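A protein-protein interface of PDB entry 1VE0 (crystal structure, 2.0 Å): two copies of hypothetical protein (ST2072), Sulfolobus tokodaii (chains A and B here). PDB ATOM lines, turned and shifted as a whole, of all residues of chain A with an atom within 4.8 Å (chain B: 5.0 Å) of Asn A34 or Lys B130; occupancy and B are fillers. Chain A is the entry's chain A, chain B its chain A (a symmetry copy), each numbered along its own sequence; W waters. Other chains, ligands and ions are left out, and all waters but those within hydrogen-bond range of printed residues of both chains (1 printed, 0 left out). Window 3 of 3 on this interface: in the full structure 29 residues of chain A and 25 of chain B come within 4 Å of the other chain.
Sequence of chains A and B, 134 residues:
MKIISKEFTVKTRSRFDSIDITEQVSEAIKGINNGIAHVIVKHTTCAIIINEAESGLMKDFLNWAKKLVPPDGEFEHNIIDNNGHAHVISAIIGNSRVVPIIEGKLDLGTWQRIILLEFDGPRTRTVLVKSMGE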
ATOM      1  N   ILE A  32      25.711  -9.179  -7.131  1.00  0.00           N
ATOM      2  CA  ILE A  32      24.888  -8.259  -7.908  1.00  0.00           C
ATOM      3  C   ILE A  32      24.496  -7.069  -7.025  1.00  0.00           C
ATOM      4  O   ILE A  32      24.030  -7.244  -5.899  1.00  0.00           O
ATOM      5  CB  ILE A  32      23.597  -8.952  -8.412  1.00  0.00           C
ATOM      6  CG1 ILE A  32      23.954 -10.077  -9.396  1.00  0.00           C
ATOM      7  CG2 ILE A  32      22.664  -7.924  -9.040  1.00  0.00           C
ATOM      8  CD1 ILE A  32      24.606  -9.607 -10.689  1.00  0.00           C
ATOM      9  N   ASN A  33      24.693  -5.863  -7.546  1.00  0.00           N
ATOM     10  CA  ASN A  33      24.376  -4.636  -6.826  1.00  0.00           C
ATOM     11  C   ASN A  33      23.006  -4.055  -7.181  1.00  0.00           C
ATOM     12  O   ASN A  33      22.273  -3.590  -6.308  1.00  0.00           O
ATOM     13  CB  ASN A  33      25.473  -3.589  -7.095  1.00  0.00           C
ATOM     14  CG  ASN A  33      25.039  -2.180  -6.733  1.00  0.00           C
ATOM     15  OD1 ASN A  33      24.387  -1.490  -7.525  1.00  0.00           O
ATOM     16  ND2 ASN A  33      25.386  -1.748  -5.523  1.00  0.00           N
ATOM     17  N   ASN A  34      22.667  -4.078  -8.465  1.00  0.00           N
ATOM     18  CA  ASN A  34      21.394  -3.544  -8.937  1.00  0.00           C
ATOM     19  C   ASN A  34      20.923  -4.470 -10.046  1.00  0.00           C
ATOM     20  O   ASN A  34      21.654  -4.717 -11.007  1.00  0.00           O
ATOM     21  CB  ASN A  34      21.599  -2.128  -9.488  1.00  0.00           C
ATOM     22  CG  ASN A  34      20.322  -1.512 -10.061  1.00  0.00           C
ATOM     23  OD1 ASN A  34      20.388  -0.584 -10.869  1.00  0.00           O
ATOM     24  ND2 ASN A  34      19.165  -2.005  -9.634  1.00  0.00           N
ATOM     25  N   GLY A  35      19.709  -4.991  -9.920  1.00  0.00           N
ATOM     26  CA  GLY A  35      19.227  -5.886 -10.956  1.00  0.00           C
ATOM     27  C   GLY A  35      18.028  -6.711 -10.568  1.00  0.00           C
ATOM     28  O   GLY A  35      17.166  -6.249  -9.822  1.00  0.00           O
ATOM     29  N   ILE A  36      17.985  -7.947 -11.063  1.00  0.00           N
ATOM     30  CA  ILE A  36      16.856  -8.834 -10.802  1.00  0.00           C
ATOM     31  C   ILE A  36      17.311 -10.220 -10.350  1.00  0.00           C
ATOM     32  O   ILE A  36      18.248 -10.789 -10.897  1.00  0.00           O
ATOM     33  CB  ILE A  36      15.984  -8.999 -12.084  1.00  0.00           C
ATOM     34  CG1 ILE A  36      15.294  -7.673 -12.429  1.00  0.00           C
ATOM     35  CG2 ILE A  36      14.951 -10.099 -11.887  1.00  0.00           C
ATOM     36  CD1 ILE A  36      14.294  -7.217 -11.378  1.00  0.00           C
ATOM     37  N   PRO A 100      13.428  -7.688  -7.081  1.00  0.00           N
ATOM     38  CA  PRO A 100      14.437  -6.735  -7.543  1.00  0.00           C
ATOM     39  C   PRO A 100      15.554  -6.631  -6.515  1.00  0.00           C
ATOM     40  O   PRO A 100      15.346  -6.901  -5.336  1.00  0.00           O
ATOM     41  CB  PRO A 100      13.655  -5.432  -7.687  1.00  0.00           C
ATOM     42  CG  PRO A 100      12.568  -5.571  -6.621  1.00  0.00           C
ATOM     43  CD  PRO A 100      12.158  -7.028  -6.730  1.00  0.00           C
ATOM     44  N   ILE A 101      16.735  -6.252  -6.988  1.00  0.00           N
ATOM     45  CA  ILE A 101      17.899  -6.079  -6.143  1.00  0.00           C
ATOM     46  C   ILE A 101      18.304  -4.613  -6.285  1.00  0.00           C
ATOM     47  O   ILE A 101      18.372  -4.098  -7.398  1.00  0.00           O
ATOM     48  CB  ILE A 101      19.086  -6.950  -6.622  1.00  0.00           C
ATOM     49  CG1 ILE A 101      18.692  -8.428  -6.619  1.00  0.00           C
ATOM     50  CG2 ILE A 101      20.293  -6.718  -5.712  1.00  0.00           C
ATOM     51  CD1 ILE A 101      19.755  -9.344  -7.210  1.00  0.00           C
ATOM     52  N   ILE A 102      18.559  -3.946  -5.167  1.00  0.00           N
ATOM     53  CA  ILE A 102      18.969  -2.551  -5.215  1.00  0.00           C
ATOM     54  C   ILE A 102      19.942  -2.324  -4.056  1.00  0.00           C
ATOM     55  O   ILE A 102      19.723  -2.804  -2.946  1.00  0.00           O
ATOM     56  CB  ILE A 102      17.730  -1.607  -5.123  1.00  0.00           C
ATOM     57  CG1 ILE A 102      18.137  -0.160  -5.417  1.00  0.00           C
ATOM     58  CG2 ILE A 102      17.090  -1.694  -3.755  1.00  0.00           C
ATOM     59  CD1 ILE A 102      18.630   0.065  -6.843  1.00  0.00           C
ATOM     60  N   MET A 132      20.774 -11.223 -12.292  1.00  0.00           N
ATOM     61  CA  MET A 132      21.369 -10.490 -13.396  1.00  0.00           C
ATOM     62  C   MET A 132      21.265  -8.996 -13.130  1.00  0.00           C
ATOM     63  O   MET A 132      20.278  -8.518 -12.577  1.00  0.00           O
ATOM     64  CB  MET A 132      20.672 -10.842 -14.726  1.00  0.00           C
ATOM     65  CG  MET A 132      21.001 -12.242 -15.249  1.00  0.00           C
ATOM     66  SD  MET A 132      20.293 -12.652 -17.038  1.00  0.00           S
ATOM     67  CE  MET A 132      20.258 -10.864 -17.764  1.00  0.00           C
ATOM     68  N   GLY A 133      22.301  -8.262 -13.523  1.00  0.00           N
ATOM     69  CA  GLY A 133      22.304  -6.823 -13.327  1.00  0.00           C
ATOM     70  C   GLY A 133      23.738  -6.361 -13.293  1.00  0.00           C
ATOM     71  O   GLY A 133      24.596  -6.988 -13.915  1.00  0.00           O
ATOM     72  N   GLU A 134      24.017  -5.291 -12.560  1.00  0.00           N
ATOM     73  CA  GLU A 134      25.386  -4.793 -12.482  1.00  0.00           C
ATOM     74  C   GLU A 134      25.923  -4.968 -11.069  1.00  0.00           C
ATOM     75  O   GLU A 134      25.100  -5.166 -10.160  1.00  0.00           O
ATOM     76  CB  GLU A 134      25.424  -3.317 -12.870  1.00  0.00           C
ATOM     77  CG  GLU A 134      24.834  -2.419 -11.814  1.00  0.00           C
ATOM     78  CD  GLU A 134      24.751  -0.977 -12.252  1.00  0.00           C
ATOM     79  OE1 GLU A 134      24.638  -0.107 -11.357  1.00  0.00           O
ATOM     80  OE2 GLU A 134      24.792  -0.720 -13.479  1.00  0.00           O
ATOM     81  OXT GLU A 134      27.156  -4.903 -10.886  1.00  0.00           O
ATOM     82  N   ILE B   3      19.837  -0.495 -16.820  1.00  0.00           N
ATOM     83  CA  ILE B   3      18.811  -0.813 -15.823  1.00  0.00           C
ATOM     84  C   ILE B   3      18.004   0.416 -15.435  1.00  0.00           C
ATOM     85  O   ILE B   3      18.556   1.387 -14.921  1.00  0.00           O
ATOM     86  CB  ILE B   3      19.431  -1.368 -14.531  1.00  0.00           C
ATOM     87  CG1 ILE B   3      20.260  -2.612 -14.848  1.00  0.00           C
ATOM     88  CG2 ILE B   3      18.325  -1.683 -13.518  1.00  0.00           C
ATOM     89  CD1 ILE B   3      21.059  -3.131 -13.674  1.00  0.00           C
ATOM     90  N   ILE B   4      16.702   0.375 -15.685  1.00  0.00           N
ATOM     91  CA  ILE B   4      15.839   1.485 -15.334  1.00  0.00           C
ATOM     92  C   ILE B   4      14.929   1.030 -14.202  1.00  0.00           C
ATOM     93  O   ILE B   4      14.388  -0.082 -14.232  1.00  0.00           O
ATOM     94  CB  ILE B   4      14.955   1.941 -16.527  1.00  0.00           C
ATOM     95  CG1 ILE B   4      15.825   2.439 -17.682  1.00  0.00           C
ATOM     96  CG2 ILE B   4      14.018   3.042 -16.079  1.00  0.00           C
ATOM     97  CD1 ILE B   4      16.702   3.612 -17.335  1.00  0.00           C
ATOM     98  N   SER B   5      14.775   1.885 -13.201  1.00  0.00           N
ATOM     99  CA  SER B   5      13.927   1.575 -12.061  1.00  0.00           C
ATOM    100  C   SER B   5      13.036   2.773 -11.824  1.00  0.00           C
ATOM    101  O   SER B   5      13.525   3.854 -11.484  1.00  0.00           O
ATOM    102  CB  SER B   5      14.772   1.318 -10.813  1.00  0.00           C
ATOM    103  OG  SER B   5      15.723   0.298 -11.044  1.00  0.00           O
ATOM    104  N   ILE B  36      13.415  -6.247 -21.256  1.00  0.00           N
ATOM    105  CA  ILE B  36      12.318  -6.769 -20.448  1.00  0.00           C
ATOM    106  C   ILE B  36      11.916  -5.802 -19.337  1.00  0.00           C
ATOM    107  O   ILE B  36      12.761  -5.214 -18.672  1.00  0.00           O
ATOM    108  CB  ILE B  36      12.721  -8.126 -19.793  1.00  0.00           C
ATOM    109  CG1 ILE B  36      12.885  -9.206 -20.870  1.00  0.00           C
ATOM    110  CG2 ILE B  36      11.679  -8.553 -18.769  1.00  0.00           C
ATOM    111  CD1 ILE B  36      11.593  -9.536 -21.602  1.00  0.00           C
ATOM    112  N   ALA B  37      10.614  -5.634 -19.174  1.00  0.00           N
ATOM    113  CA  ALA B  37      10.066  -4.794 -18.127  1.00  0.00           C
ATOM    114  C   ALA B  37       9.472  -5.738 -17.094  1.00  0.00           C
ATOM    115  O   ALA B  37       8.655  -6.602 -17.429  1.00  0.00           O
ATOM    116  CB  ALA B  37       8.969  -3.894 -18.690  1.00  0.00           C
ATOM    117  N   HIS B  38       9.912  -5.606 -15.853  1.00  0.00           N
ATOM    118  CA  HIS B  38       9.355  -6.414 -14.779  1.00  0.00           C
ATOM    119  C   HIS B  38       8.417  -5.471 -14.041  1.00  0.00           C
ATOM    120  O   HIS B  38       8.871  -4.502 -13.443  1.00  0.00           O
ATOM    121  CB  HIS B  38      10.455  -6.880 -13.829  1.00  0.00           C
ATOM    122  CG  HIS B  38      11.413  -7.844 -14.448  1.00  0.00           C
ATOM    123  ND1 HIS B  38      11.187  -9.203 -14.473  1.00  0.00           N
ATOM    124  CD2 HIS B  38      12.587  -7.644 -15.094  1.00  0.00           C
ATOM    125  CE1 HIS B  38      12.180  -9.800 -15.108  1.00  0.00           C
ATOM    126  NE2 HIS B  38      13.043  -8.877 -15.493  1.00  0.00           N
ATOM    127  N   ILE B  40       6.348  -4.921 -11.048  1.00  0.00           N
ATOM    128  CA  ILE B  40       6.334  -5.474  -9.697  1.00  0.00           C
ATOM    129  C   ILE B  40       5.639  -4.648  -8.629  1.00  0.00           C
ATOM    130  O   ILE B  40       5.731  -3.426  -8.635  1.00  0.00           O
ATOM    131  CB  ILE B  40       7.814  -5.658  -9.223  1.00  0.00           C
ATOM    132  CG1 ILE B  40       8.544  -6.610 -10.164  1.00  0.00           C
ATOM    133  CG2 ILE B  40       7.880  -6.136  -7.760  1.00  0.00           C
ATOM    134  CD1 ILE B  40      10.030  -6.334 -10.237  1.00  0.00           C
ATOM    135  N   LEU B 128       6.345  -0.868  -9.062  1.00  0.00           N
ATOM    136  CA  LEU B 128       7.727  -0.678  -9.491  1.00  0.00           C
ATOM    137  C   LEU B 128       7.916  -1.307 -10.876  1.00  0.00           C
ATOM    138  O   LEU B 128       7.534  -2.468 -11.100  1.00  0.00           O
ATOM    139  CB  LEU B 128       8.699  -1.342  -8.505  1.00  0.00           C
ATOM    140  CG  LEU B 128      10.117  -1.612  -9.020  1.00  0.00           C
ATOM    141  CD1 LEU B 128      10.877  -0.299  -9.253  1.00  0.00           C
ATOM    142  CD2 LEU B 128      10.851  -2.485  -8.008  1.00  0.00           C
ATOM    143  N   VAL B 129       8.466  -0.539 -11.811  1.00  0.00           N
ATOM    144  CA  VAL B 129       8.753  -1.062 -13.137  1.00  0.00           C
ATOM    145  C   VAL B 129      10.275  -1.057 -13.241  1.00  0.00           C
ATOM    146  O   VAL B 129      10.924  -0.004 -13.296  1.00  0.00           O
ATOM    147  CB  VAL B 129       8.151  -0.201 -14.268  1.00  0.00           C
ATOM    148  CG1 VAL B 129       8.464  -0.857 -15.623  1.00  0.00           C
ATOM    149  CG2 VAL B 129       6.627  -0.069 -14.082  1.00  0.00           C
ATOM    150  N   LYS B 130      10.842  -2.251 -13.233  1.00  0.00           N
ATOM    151  CA  LYS B 130      12.279  -2.424 -13.296  1.00  0.00           C
ATOM    152  C   LYS B 130      12.565  -3.009 -14.664  1.00  0.00           C
ATOM    153  O   LYS B 130      12.239  -4.170 -14.928  1.00  0.00           O
ATOM    154  CB  LYS B 130      12.715  -3.396 -12.194  1.00  0.00           C
ATOM    155  CG  LYS B 130      14.208  -3.555 -12.038  1.00  0.00           C
ATOM    156  CD  LYS B 130      14.650  -3.066 -10.687  1.00  0.00           C
ATOM    157  CE  LYS B 130      16.111  -3.350 -10.446  1.00  0.00           C
ATOM    158  NZ  LYS B 130      16.594  -2.574  -9.286  1.00  0.00           N
ATOM    159  N   SER B 131      13.162  -2.203 -15.536  1.00  0.00           N
ATOM    160  CA  SER B 131      13.460  -2.650 -16.887  1.00  0.00           C
ATOM    161  C   SER B 131      14.941  -2.862 -17.130  1.00  0.00           C
ATOM    162  O   SER B 131      15.789  -2.130 -16.609  1.00  0.00           O
ATOM    163  CB  SER B 131      12.917  -1.642 -17.902  1.00  0.00           C
ATOM    164  OG  SER B 131      11.557  -1.371 -17.648  1.00  0.00           O
ATOM    165  N   MET B 132      15.243  -3.869 -17.935  1.00  0.00           N
ATOM    166  CA  MET B 132      16.618  -4.196 -18.273  1.00  0.00           C
ATOM    167  C   MET B 132      16.716  -4.517 -19.757  1.00  0.00           C
ATOM    168  O   MET B 132      15.814  -5.117 -20.336  1.00  0.00           O
ATOM    169  CB  MET B 132      17.118  -5.392 -17.438  1.00  0.00           C
ATOM    170  CG  MET B 132      17.375  -5.059 -15.966  1.00  0.00           C
ATOM    171  SD  MET B 132      18.202  -6.502 -14.916  1.00  0.00           S
ATOM    172  CE  MET B 132      19.163  -7.392 -16.333  1.00  0.00           C
HETATM  173  O   HOH W   1      18.268   1.325 -11.529  1.00  0.00           O
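Met A132 touches its own counterpart, Met B132. 2 positions are printed for both chains. Of the 11 pairs that touch across the chains among the printed residues, 1 has its exchanged pair printed and touching as well.
Among the printed residues, merely in contact across the chains: Asn A34 with Ile B3 (3.2 Å), Gly A35 with Lys B130 (3.1 Å), Ile A36 with His B38 (3.8 Å), Ile A36 with Lys B130 (3.7 Å), Pro A100 with Leu B128 (3.8 Å), Pro A100 with Lys B130 (3.9 Å), Gly A133 with Ile B3 (3.9 Å) and Glu A134 with Ile B3 (3.8 Å).
Asn A33 touches none of the printed residues of chain B. Asn A34 touches just these residues of chain B: Ile B3 (3.2 Å) and Lys B130 (2.7 Å). Of the printed residues of chain B, Ile A101 touches Lys B130. Printed residues of chain B within 4 Å of Met A132: Met B132 (3.7 Å). Of the printed residues of chain B, Gly A133 touches Ile B3. Ser B131 touches none of the printed residues of chain A. The nearest residue of chain B that does not touch Asn A34 is Ser B5 (4.4 Å). The nearest residue of chain A that does not touch Lys B130 is Ile A102 (4.1 Å).
The backbone carbonyl oxygen of Ile A101 is in hydrogen-bond range of the side-chain amide nitrogen of Asn A34 (3.2 Å). The backbone carbonyl oxygen of Asn A34 lies within hydrogen-bond range of the backbone NH of Glu A134 (2.9 Å). O of Gly A35 is in hydrogen-bond range of N of Ile A101 (2.9 Å). NZ of Lys B130 is in hydrogen-bond range of OG of Ser B5 (3.5 Å). O of Met B132 lies within hydrogen-bond range of N of Ile B36, 2.8 Å away. The backbone carbonyl oxygen of Ile B40 is in hydrogen-bond range of the backbone NH of Leu B128 (2.7 Å).
Printed residues of chain B that touch a printed residue of chain A: Ile B3, His B38, Leu B128, Lys B130 and Met B132. Of the 11 printed residues of chain A, 8 touch a printed residue of chain B. Hydrophobic or aromatic side chains of chain A that line the printed part of chain B: Ile A36, Pro A100 and Met A132. Among the printed residues, 11 pairs touch across the chains. Among the printed residues, no Asp or Glu carboxylate lies within 4 Å of a Lys or Arg side-chain nitrogen of the other chain.
NZ of Lys B130 lies close to ND2 of Asn A34. O of Ile A101 is in hydrogen-bond range of NZ of Lys B130, at 3.0 Å. SD of Met B132 sits close to O of Met A132 (3.7 Å).
Water W1 lies within hydrogen-bond range of OG of Ser B5 (2.8 Å), OD1 of Asn A34 (2.9 Å) and O of Ile B3 (3.4 Å).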
